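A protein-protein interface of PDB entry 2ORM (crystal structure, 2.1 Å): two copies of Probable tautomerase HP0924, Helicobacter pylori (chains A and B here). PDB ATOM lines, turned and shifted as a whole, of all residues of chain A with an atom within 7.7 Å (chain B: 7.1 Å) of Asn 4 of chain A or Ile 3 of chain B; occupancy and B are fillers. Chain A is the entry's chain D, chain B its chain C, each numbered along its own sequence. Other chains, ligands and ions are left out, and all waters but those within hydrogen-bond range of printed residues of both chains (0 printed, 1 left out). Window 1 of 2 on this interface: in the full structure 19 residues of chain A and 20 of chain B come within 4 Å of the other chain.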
ATOM      1  N   PHE A   2      14.953   1.041 -36.789  1.00  0.00           N
ATOM      2  CA  PHE A   2      16.226   0.832 -36.098  1.00  0.00           C
ATOM      3  C   PHE A   2      16.531   2.015 -35.158  1.00  0.00           C
ATOM      4  O   PHE A   2      16.489   3.173 -35.574  1.00  0.00           O
ATOM      5  CB  PHE A   2      17.344   0.693 -37.144  1.00  0.00           C
ATOM      6  CG  PHE A   2      18.735   0.666 -36.566  1.00  0.00           C
ATOM      7  CD1 PHE A   2      19.197  -0.447 -35.877  1.00  0.00           C
ATOM      8  CD2 PHE A   2      19.587   1.760 -36.721  1.00  0.00           C
ATOM      9  CE1 PHE A   2      20.489  -0.481 -35.352  1.00  0.00           C
ATOM     10  CE2 PHE A   2      20.883   1.742 -36.202  1.00  0.00           C
ATOM     11  CZ  PHE A   2      21.335   0.617 -35.512  1.00  0.00           C
ATOM     12  N   ILE A   3      16.836   1.713 -33.900  1.00  0.00           N
ATOM     13  CA  ILE A   3      17.152   2.742 -32.903  1.00  0.00           C
ATOM     14  C   ILE A   3      18.498   2.434 -32.242  1.00  0.00           C
ATOM     15  O   ILE A   3      18.703   1.337 -31.715  1.00  0.00           O
ATOM     16  CB  ILE A   3      16.060   2.825 -31.789  1.00  0.00           C
ATOM     17  CG1 ILE A   3      14.692   3.129 -32.407  1.00  0.00           C
ATOM     18  CG2 ILE A   3      16.410   3.917 -30.775  1.00  0.00           C
ATOM     19  CD1 ILE A   3      13.967   1.904 -32.941  1.00  0.00           C
ATOM     20  N   ASN A   4      19.413   3.399 -32.283  1.00  0.00           N
ATOM     21  CA  ASN A   4      20.743   3.251 -31.691  1.00  0.00           C
ATOM     22  C   ASN A   4      20.842   4.278 -30.553  1.00  0.00           C
ATOM     23  O   ASN A   4      20.619   5.471 -30.768  1.00  0.00           O
ATOM     24  CB  ASN A   4      21.811   3.527 -32.762  1.00  0.00           C
ATOM     25  CG  ASN A   4      23.227   3.183 -32.308  1.00  0.00           C
ATOM     26  OD1 ASN A   4      24.198   3.653 -32.906  1.00  0.00           O
ATOM     27  ND2 ASN A   4      23.356   2.355 -31.271  1.00  0.00           N
ATOM     28  N   ILE A   5      21.171   3.809 -29.352  1.00  0.00           N
ATOM     29  CA  ILE A   5      21.278   4.667 -28.176  1.00  0.00           C
ATOM     30  C   ILE A   5      22.700   4.628 -27.640  1.00  0.00           C
ATOM     31  O   ILE A   5      23.182   3.563 -27.273  1.00  0.00           O
ATOM     32  CB  ILE A   5      20.327   4.187 -27.031  1.00  0.00           C
ATOM     33  CG1 ILE A   5      18.872   4.242 -27.485  1.00  0.00           C
ATOM     34  CG2 ILE A   5      20.512   5.054 -25.780  1.00  0.00           C
ATOM     35  CD1 ILE A   5      17.900   3.620 -26.468  1.00  0.00           C
ATOM     36  N   LYS A   6      23.365   5.784 -27.599  1.00  0.00           N
ATOM     37  CA  LYS A   6      24.734   5.881 -27.084  1.00  0.00           C
ATOM     38  C   LYS A   6      24.746   6.700 -25.782  1.00  0.00           C
ATOM     39  O   LYS A   6      24.347   7.861 -25.782  1.00  0.00           O
ATOM     40  CB  LYS A   6      25.639   6.551 -28.125  1.00  0.00           C
ATOM     41  CG  LYS A   6      25.849   5.734 -29.390  1.00  0.00           C
ATOM     42  CD  LYS A   6      26.627   6.511 -30.432  1.00  0.00           C
ATOM     43  CE  LYS A   6      26.893   5.674 -31.670  1.00  0.00           C
ATOM     44  NZ  LYS A   6      27.671   4.442 -31.336  1.00  0.00           N
ATOM     45  N   LEU A   7      25.213   6.111 -24.681  1.00  0.00           N
ATOM     46  CA  LEU A   7      25.219   6.830 -23.405  1.00  0.00           C
ATOM     47  C   LEU A   7      26.431   6.551 -22.513  1.00  0.00           C
ATOM     48  O   LEU A   7      27.137   5.569 -22.721  1.00  0.00           O
ATOM     49  CB  LEU A   7      23.927   6.512 -22.648  1.00  0.00           C
ATOM     50  CG  LEU A   7      23.664   5.044 -22.313  1.00  0.00           C
ATOM     51  CD1 LEU A   7      24.380   4.681 -21.009  1.00  0.00           C
ATOM     52  CD2 LEU A   7      22.166   4.798 -22.190  1.00  0.00           C
ATOM     53  N   VAL A  26      11.234   2.268 -25.505  1.00  0.00           N
ATOM     54  CA  VAL A  26      11.359   2.816 -26.852  1.00  0.00           C
ATOM     55  C   VAL A  26      10.514   2.046 -27.860  1.00  0.00           C
ATOM     56  O   VAL A  26       9.988   2.624 -28.812  1.00  0.00           O
ATOM     57  CB  VAL A  26      12.841   2.817 -27.315  1.00  0.00           C
ATOM     58  CG1 VAL A  26      12.935   3.153 -28.787  1.00  0.00           C
ATOM     59  CG2 VAL A  26      13.633   3.837 -26.514  1.00  0.00           C
ATOM     60  N   VAL A  42      14.422  -3.046 -33.889  1.00  0.00           N
ATOM     61  CA  VAL A  42      15.763  -3.385 -33.422  1.00  0.00           C
ATOM     62  C   VAL A  42      16.341  -2.223 -32.620  1.00  0.00           C
ATOM     63  O   VAL A  42      16.287  -1.072 -33.046  1.00  0.00           O
ATOM     64  CB  VAL A  42      16.719  -3.694 -34.605  1.00  0.00           C
ATOM     65  CG1 VAL A  42      18.115  -4.009 -34.082  1.00  0.00           C
ATOM     66  CG2 VAL A  42      16.188  -4.859 -35.416  1.00  0.00           C
ATOM     67  N   VAL A  43      16.897  -2.527 -31.457  1.00  0.00           N
ATOM     68  CA  VAL A  43      17.473  -1.498 -30.613  1.00  0.00           C
ATOM     69  C   VAL A  43      18.875  -1.895 -30.177  1.00  0.00           C
ATOM     70  O   VAL A  43      19.126  -3.035 -29.773  1.00  0.00           O
ATOM     71  CB  VAL A  43      16.600  -1.249 -29.353  1.00  0.00           C
ATOM     72  CG1 VAL A  43      17.275  -0.225 -28.438  1.00  0.00           C
ATOM     73  CG2 VAL A  43      15.213  -0.737 -29.769  1.00  0.00           C
ATOM     74  N   ILE A  44      19.802  -0.951 -30.276  1.00  0.00           N
ATOM     75  CA  ILE A  44      21.168  -1.214 -29.864  1.00  0.00           C
ATOM     76  C   ILE A  44      21.633  -0.115 -28.911  1.00  0.00           C
ATOM     77  O   ILE A  44      21.549   1.075 -29.223  1.00  0.00           O
ATOM     78  CB  ILE A  44      22.116  -1.296 -31.094  1.00  0.00           C
ATOM     79  CG1 ILE A  44      21.786  -2.556 -31.911  1.00  0.00           C
ATOM     80  CG2 ILE A  44      23.569  -1.306 -30.643  1.00  0.00           C
ATOM     81  CD1 ILE A  44      22.689  -2.775 -33.122  1.00  0.00           C
ATOM     82  N   ILE A  45      22.103  -0.523 -27.739  1.00  0.00           N
ATOM     83  CA  ILE A  45      22.595   0.419 -26.741  1.00  0.00           C
ATOM     84  C   ILE A  45      24.118   0.335 -26.673  1.00  0.00           C
ATOM     85  O   ILE A  45      24.678  -0.738 -26.445  1.00  0.00           O
ATOM     86  CB  ILE A  45      21.976   0.115 -25.355  1.00  0.00           C
ATOM     87  CG1 ILE A  45      20.451   0.273 -25.439  1.00  0.00           C
ATOM     88  CG2 ILE A  45      22.543   1.066 -24.293  1.00  0.00           C
ATOM     89  CD1 ILE A  45      19.682  -0.331 -24.277  1.00  0.00           C
ATOM     90  N   ASP A  46      24.786   1.459 -26.919  1.00  0.00           N
ATOM     91  CA  ASP A  46      26.248   1.514 -26.859  1.00  0.00           C
ATOM     92  C   ASP A  46      26.640   2.297 -25.605  1.00  0.00           C
ATOM     93  O   ASP A  46      26.135   3.396 -25.365  1.00  0.00           O
ATOM     94  CB  ASP A  46      26.846   2.231 -28.090  1.00  0.00           C
ATOM     95  CG  ASP A  46      26.681   1.442 -29.387  1.00  0.00           C
ATOM     96  OD1 ASP A  46      26.972   0.232 -29.397  1.00  0.00           O
ATOM     97  OD2 ASP A  46      26.277   2.037 -30.410  1.00  0.00           O
ATOM     98  N   TYR A  53      33.412  10.749 -24.874  1.00  0.00           N
ATOM     99  CA  TYR A  53      32.167  11.453 -25.171  1.00  0.00           C
ATOM    100  C   TYR A  53      32.404  12.938 -24.916  1.00  0.00           C
ATOM    101  O   TYR A  53      32.700  13.343 -23.789  1.00  0.00           O
ATOM    102  CB  TYR A  53      31.048  10.931 -24.252  1.00  0.00           C
ATOM    103  CG  TYR A  53      29.631  11.258 -24.691  1.00  0.00           C
ATOM    104  CD1 TYR A  53      28.768  10.243 -25.107  1.00  0.00           C
ATOM    105  CD2 TYR A  53      29.148  12.572 -24.681  1.00  0.00           C
ATOM    106  CE1 TYR A  53      27.462  10.518 -25.500  1.00  0.00           C
ATOM    107  CE2 TYR A  53      27.834  12.866 -25.076  1.00  0.00           C
ATOM    108  CZ  TYR A  53      26.997  11.827 -25.482  1.00  0.00           C
ATOM    109  OH  TYR A  53      25.694  12.070 -25.854  1.00  0.00           O
ATOM    110  N   PRO B   1      23.265  11.927 -23.729  1.00  0.00           N
ATOM    111  CA  PRO B   1      23.166  10.691 -24.551  1.00  0.00           C
ATOM    112  C   PRO B   1      22.710  11.009 -25.971  1.00  0.00           C
ATOM    113  O   PRO B   1      22.039  12.015 -26.200  1.00  0.00           O
ATOM    114  CB  PRO B   1      22.162   9.777 -23.856  1.00  0.00           C
ATOM    115  CG  PRO B   1      21.259  10.802 -23.164  1.00  0.00           C
ATOM    116  CD  PRO B   1      22.218  11.925 -22.686  1.00  0.00           C
ATOM    117  N   PHE B   2      23.074  10.140 -26.912  1.00  0.00           N
ATOM    118  CA  PHE B   2      22.720  10.304 -28.322  1.00  0.00           C
ATOM    119  C   PHE B   2      21.766   9.194 -28.770  1.00  0.00           C
ATOM    120  O   PHE B   2      21.974   8.027 -28.455  1.00  0.00           O
ATOM    121  CB  PHE B   2      23.995  10.271 -29.174  1.00  0.00           C
ATOM    122  CG  PHE B   2      23.753  10.374 -30.653  1.00  0.00           C
ATOM    123  CD1 PHE B   2      23.362  11.578 -31.231  1.00  0.00           C
ATOM    124  CD2 PHE B   2      23.921   9.263 -31.479  1.00  0.00           C
ATOM    125  CE1 PHE B   2      23.156  11.678 -32.611  1.00  0.00           C
ATOM    126  CE2 PHE B   2      23.714   9.353 -32.859  1.00  0.00           C
ATOM    127  CZ  PHE B   2      23.328  10.560 -33.423  1.00  0.00           C
ATOM    128  N   ILE B   3      20.718   9.564 -29.501  1.00  0.00           N
ATOM    129  CA  ILE B   3      19.749   8.588 -29.991  1.00  0.00           C
ATOM    130  C   ILE B   3      19.492   8.777 -31.494  1.00  0.00           C
ATOM    131  O   ILE B   3      19.042   9.835 -31.928  1.00  0.00           O
ATOM    132  CB  ILE B   3      18.385   8.688 -29.235  1.00  0.00           C
ATOM    133  CG1 ILE B   3      18.565   8.354 -27.748  1.00  0.00           C
ATOM    134  CG2 ILE B   3      17.379   7.706 -29.836  1.00  0.00           C
ATOM    135  CD1 ILE B   3      18.702   9.587 -26.844  1.00  0.00           C
ATOM    136  N   ASN B   4      19.774   7.738 -32.277  1.00  0.00           N
ATOM    137  CA  ASN B   4      19.576   7.776 -33.728  1.00  0.00           C
ATOM    138  C   ASN B   4      18.440   6.813 -34.105  1.00  0.00           C
ATOM    139  O   ASN B   4      18.470   5.629 -33.764  1.00  0.00           O
ATOM    140  CB  ASN B   4      20.888   7.373 -34.435  1.00  0.00           C
ATOM    141  CG  ASN B   4      20.829   7.514 -35.961  1.00  0.00           C
ATOM    142  OD1 ASN B   4      21.635   6.904 -36.674  1.00  0.00           O
ATOM    143  ND2 ASN B   4      19.895   8.324 -36.467  1.00  0.00           N
ATOM    144  N   ILE B   5      17.437   7.324 -34.804  1.00  0.00           N
ATOM    145  CA  ILE B   5      16.307   6.505 -35.225  1.00  0.00           C
ATOM    146  C   ILE B   5      16.244   6.505 -36.759  1.00  0.00           C
ATOM    147  O   ILE B   5      16.214   7.565 -37.377  1.00  0.00           O
ATOM    148  CB  ILE B   5      14.961   7.073 -34.664  1.00  0.00           C
ATOM    149  CG1 ILE B   5      14.986   7.091 -33.132  1.00  0.00           C
ATOM    150  CG2 ILE B   5      13.793   6.240 -35.161  1.00  0.00           C
ATOM    151  CD1 ILE B   5      13.803   7.827 -32.499  1.00  0.00           C
ATOM    152  N   LYS B   6      16.272   5.314 -37.359  1.00  0.00           N
ATOM    153  CA  LYS B   6      16.176   5.168 -38.817  1.00  0.00           C
ATOM    154  C   LYS B   6      14.886   4.392 -39.084  1.00  0.00           C
ATOM    155  O   LYS B   6      14.713   3.272 -38.595  1.00  0.00           O
ATOM    156  CB  LYS B   6      17.374   4.391 -39.388  1.00  0.00           C
ATOM    157  CG  LYS B   6      18.738   5.081 -39.207  1.00  0.00           C
ATOM    158  CD  LYS B   6      19.875   4.286 -39.851  1.00  0.00           C
ATOM    159  CE  LYS B   6      21.248   4.957 -39.655  1.00  0.00           C
ATOM    160  NZ  LYS B   6      21.323   6.323 -40.260  1.00  0.00           N
ATOM    161  N   VAL B  26      11.283   9.787 -26.217  1.00  0.00           N
ATOM    162  CA  VAL B  26      12.538   9.095 -25.940  1.00  0.00           C
ATOM    163  C   VAL B  26      13.325   9.925 -24.927  1.00  0.00           C
ATOM    164  O   VAL B  26      14.008   9.378 -24.064  1.00  0.00           O
ATOM    165  CB  VAL B  26      13.407   8.901 -27.228  1.00  0.00           C
ATOM    166  CG1 VAL B  26      12.686   8.001 -28.212  1.00  0.00           C
ATOM    167  CG2 VAL B  26      13.702  10.235 -27.871  1.00  0.00           C
ATOM    168  N   SER B  27      13.223  11.247 -25.034  1.00  0.00           N
ATOM    169  CA  SER B  27      13.921  12.128 -24.101  1.00  0.00           C
ATOM    170  C   SER B  27      13.421  11.903 -22.673  1.00  0.00           C
ATOM    171  O   SER B  27      14.219  11.734 -21.753  1.00  0.00           O
ATOM    172  CB  SER B  27      13.728  13.601 -24.494  1.00  0.00           C
ATOM    173  OG  SER B  27      14.317  13.884 -25.757  1.00  0.00           O
ATOM    174  N   MET B  30      14.685   8.684 -20.915  1.00  0.00           N
ATOM    175  CA  MET B  30      16.012   8.728 -20.313  1.00  0.00           C
ATOM    176  C   MET B  30      15.944   9.359 -18.916  1.00  0.00           C
ATOM    177  O   MET B  30      16.711   8.998 -18.029  1.00  0.00           O
ATOM    178  CB  MET B  30      16.985   9.552 -21.179  1.00  0.00           C
ATOM    179  CG  MET B  30      17.221   9.049 -22.611  1.00  0.00           C
ATOM    180  SD  MET B  30      17.924   7.380 -22.741  1.00  0.00           S
ATOM    181  CE  MET B  30      16.487   6.487 -23.291  1.00  0.00           C
ATOM    182  N   ILE B  41      20.174  15.859 -24.177  1.00  0.00           N
ATOM    183  CA  ILE B  41      19.768  14.756 -25.042  1.00  0.00           C
ATOM    184  C   ILE B  41      19.651  15.123 -26.526  1.00  0.00           C
ATOM    185  O   ILE B  41      18.899  16.021 -26.895  1.00  0.00           O
ATOM    186  CB  ILE B  41      18.418  14.184 -24.551  1.00  0.00           C
ATOM    187  CG1 ILE B  41      18.511  13.904 -23.039  1.00  0.00           C
ATOM    188  CG2 ILE B  41      18.063  12.931 -25.349  1.00  0.00           C
ATOM    189  CD1 ILE B  41      17.215  13.483 -22.374  1.00  0.00           C
ATOM    190  N   VAL B  42      20.401  14.425 -27.377  1.00  0.00           N
ATOM    191  CA  VAL B  42      20.341  14.665 -28.819  1.00  0.00           C
ATOM    192  C   VAL B  42      19.658  13.480 -29.501  1.00  0.00           C
ATOM    193  O   VAL B  42      19.951  12.327 -29.204  1.00  0.00           O
ATOM    194  CB  VAL B  42      21.750  14.838 -29.444  1.00  0.00           C
ATOM    195  CG1 VAL B  42      21.626  15.001 -30.961  1.00  0.00           C
ATOM    196  CG2 VAL B  42      22.447  16.046 -28.842  1.00  0.00           C
ATOM    197  N   VAL B  43      18.738  13.775 -30.409  1.00  0.00           N
ATOM    198  CA  VAL B  43      18.001  12.744 -31.130  1.00  0.00           C
ATOM    199  C   VAL B  43      18.042  13.084 -32.620  1.00  0.00           C
ATOM    200  O   VAL B  43      17.824  14.231 -33.009  1.00  0.00           O
ATOM    201  CB  VAL B  43      16.508  12.682 -30.654  1.00  0.00           C
ATOM    202  CG1 VAL B  43      15.723  11.678 -31.494  1.00  0.00           C
ATOM    203  CG2 VAL B  43      16.433  12.297 -29.181  1.00  0.00           C
ATOM    204  N   ILE B  44      18.356  12.100 -33.454  1.00  0.00           N
ATOM    205  CA  ILE B  44      18.396  12.320 -34.900  1.00  0.00           C
ATOM    206  C   ILE B  44      17.538  11.264 -35.597  1.00  0.00           C
ATOM    207  O   ILE B  44      17.677  10.062 -35.340  1.00  0.00           O
ATOM    208  CB  ILE B  44      19.850  12.257 -35.465  1.00  0.00           C
ATOM    209  CG1 ILE B  44      20.641  13.497 -35.030  1.00  0.00           C
ATOM    210  CG2 ILE B  44      19.816  12.179 -36.996  1.00  0.00           C
ATOM    211  CD1 ILE B  44      22.072  13.554 -35.572  1.00  0.00           C
ATOM    212  N   ILE B  45      16.651  11.714 -36.475  1.00  0.00           N
ATOM    213  CA  ILE B  45      15.775  10.801 -37.199  1.00  0.00           C
ATOM    214  C   ILE B  45      16.123  10.724 -38.688  1.00  0.00           C
ATOM    215  O   ILE B  45      16.130  11.735 -39.375  1.00  0.00           O
ATOM    216  CB  ILE B  45      14.300  11.238 -37.054  1.00  0.00           C
ATOM    217  CG1 ILE B  45      13.899  11.205 -35.576  1.00  0.00           C
ATOM    218  CG2 ILE B  45      13.394  10.331 -37.887  1.00  0.00           C
ATOM    219  CD1 ILE B  45      12.527  11.795 -35.297  1.00  0.00           C
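Of the 14 printed residues of chain B, 6 touch a printed residue of chain A.
Printed residues of chain B that touch a printed residue of chain A: Pro 1, Phe 2, Ile 3, Asn 4, Ile 5 and Lys 6.
Among the printed residues, no Asp or Glu carboxylate lies within 4 Å of a Lys or Arg side-chain nitrogen of the other chain.
Phe 2 of chain A touches Asn 4 of chain B, and with the chains exchanged Asn 4 of chain A touches Phe 2 of chain B.
Phe 2 of chain A touches Lys 6 of chain B, and with the chains exchanged Lys 6 of chain A touches Phe 2 of chain B.
Ile 3 of chain A touches Asn 4 of chain B, and with the chains exchanged Asn 4 of chain A touches Ile 3 of chain B.
Asn 4 of chain B touches its own counterpart, Asn 4 of chain A.
The side-chain hydroxyl of Tyr 53 of chain A is in hydrogen-bond range of the backbone NH of Phe 2 of chain B (3.4 Å).
N of Lys 6 of chain B sits at hydrogen-bond distance from O of Phe 2 of chain A, 2.8 Å away.
OH of Tyr 53 of chain A lies close to N of Pro 1 of chain B, at 3.2 Å.
The backbone NH (N) of Lys 6 of chain A lies within hydrogen-bond range of the backbone carbonyl oxygen (O) of Phe 2 of chain B (2.8 Å).
The backbone carbonyl oxygen (O) of Asn 4 of chain B lies within hydrogen-bond range of the backbone NH (N) of Asn 4 of chain A (2.8 Å).
N of Ile 5 of chain A sits at hydrogen-bond distance from O of Ile 44 of chain A, at 2.8 Å.
The backbone carbonyl oxygen of Asp 46 of chain A lies within hydrogen-bond range of the backbone NH of Leu 7 of chain A, at 2.9 Å.
The backbone carbonyl oxygen (O) of Ile 44 of chain B is in hydrogen-bond range of the side-chain amide nitrogen (ND2) of Asn 4 of chain B, at 3.0 Å.
The side-chain amino group (NZ) of Lys 6 of chain A is in salt-bridge range of the side-chain carboxylate (OD2) of Asp 46 of chain A (2.9 Å).
The backbone NH (N) of Ile 44 of chain A sits at hydrogen-bond distance from the backbone carbonyl oxygen (O) of Ile 3 of chain A, 2.9 Å away.
O of Pro 1 of chain B sits at hydrogen-bond distance from N of Val 42 of chain B.
Asn 4 of chain B touches Phe 2 of chain A.
Phe 2 of chain A touches Ile 5 of chain B (O to CA, 3.4 Å).
Asn 4 of chain B touches Ile 3 of chain A (O to CA, 3.3 Å).
Phe 2 of chain B touches Asn 4 of chain A.
Ile 3 of chain B touches Asn 4 of chain A (CA to O, 3.3 Å).
Phe 2 of chain B touches Ile 5 of chain A.
O of Lys 6 of chain A touches CA of Pro 1 of chain B, 3.3 Å away.
Pro 1 of chain B touches Leu 7 of chain A (CB to CB, 3.9 Å).
Of the printed residues of chain B, Asn 4 of chain A touches Phe 2, Ile 3 and Asn 4.
Printed residues of chain B within 4 Å of Ile 5 of chain A: Phe 2.
Ile 45 of chain A touches none of the printed residues of chain B.
Of the printed residues of chain A, Pro 1 of chain B touches Lys 6 (3.3 Å), Leu 7 (3.9 Å) and Tyr 53 (3.2 Å).
Of the printed residues of chain A, Phe 2 of chain B touches Asn 4, Ile 5, Lys 6 and Tyr 53.
Of chain A, only Asn 4 comes within 4 Å of Ile 3 of chain B.
Printed residues of chain A within 4 Å of Ile 5 of chain B: Phe 2.
Ser 27 of chain B touches none of the printed residues of chain A.
The nearest residue of chain B that does not touch Asn 4 of chain A is Ile 5 of chain B (5.1 Å).
The nearest residue of chain A that does not touch Ile 3 of chain B is Ile 3 of chain A (4.02 Å).
The nearest printed residue of chain B that does not touch Leu 7 of chain A is Met 30 of chain B (5.0 Å).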
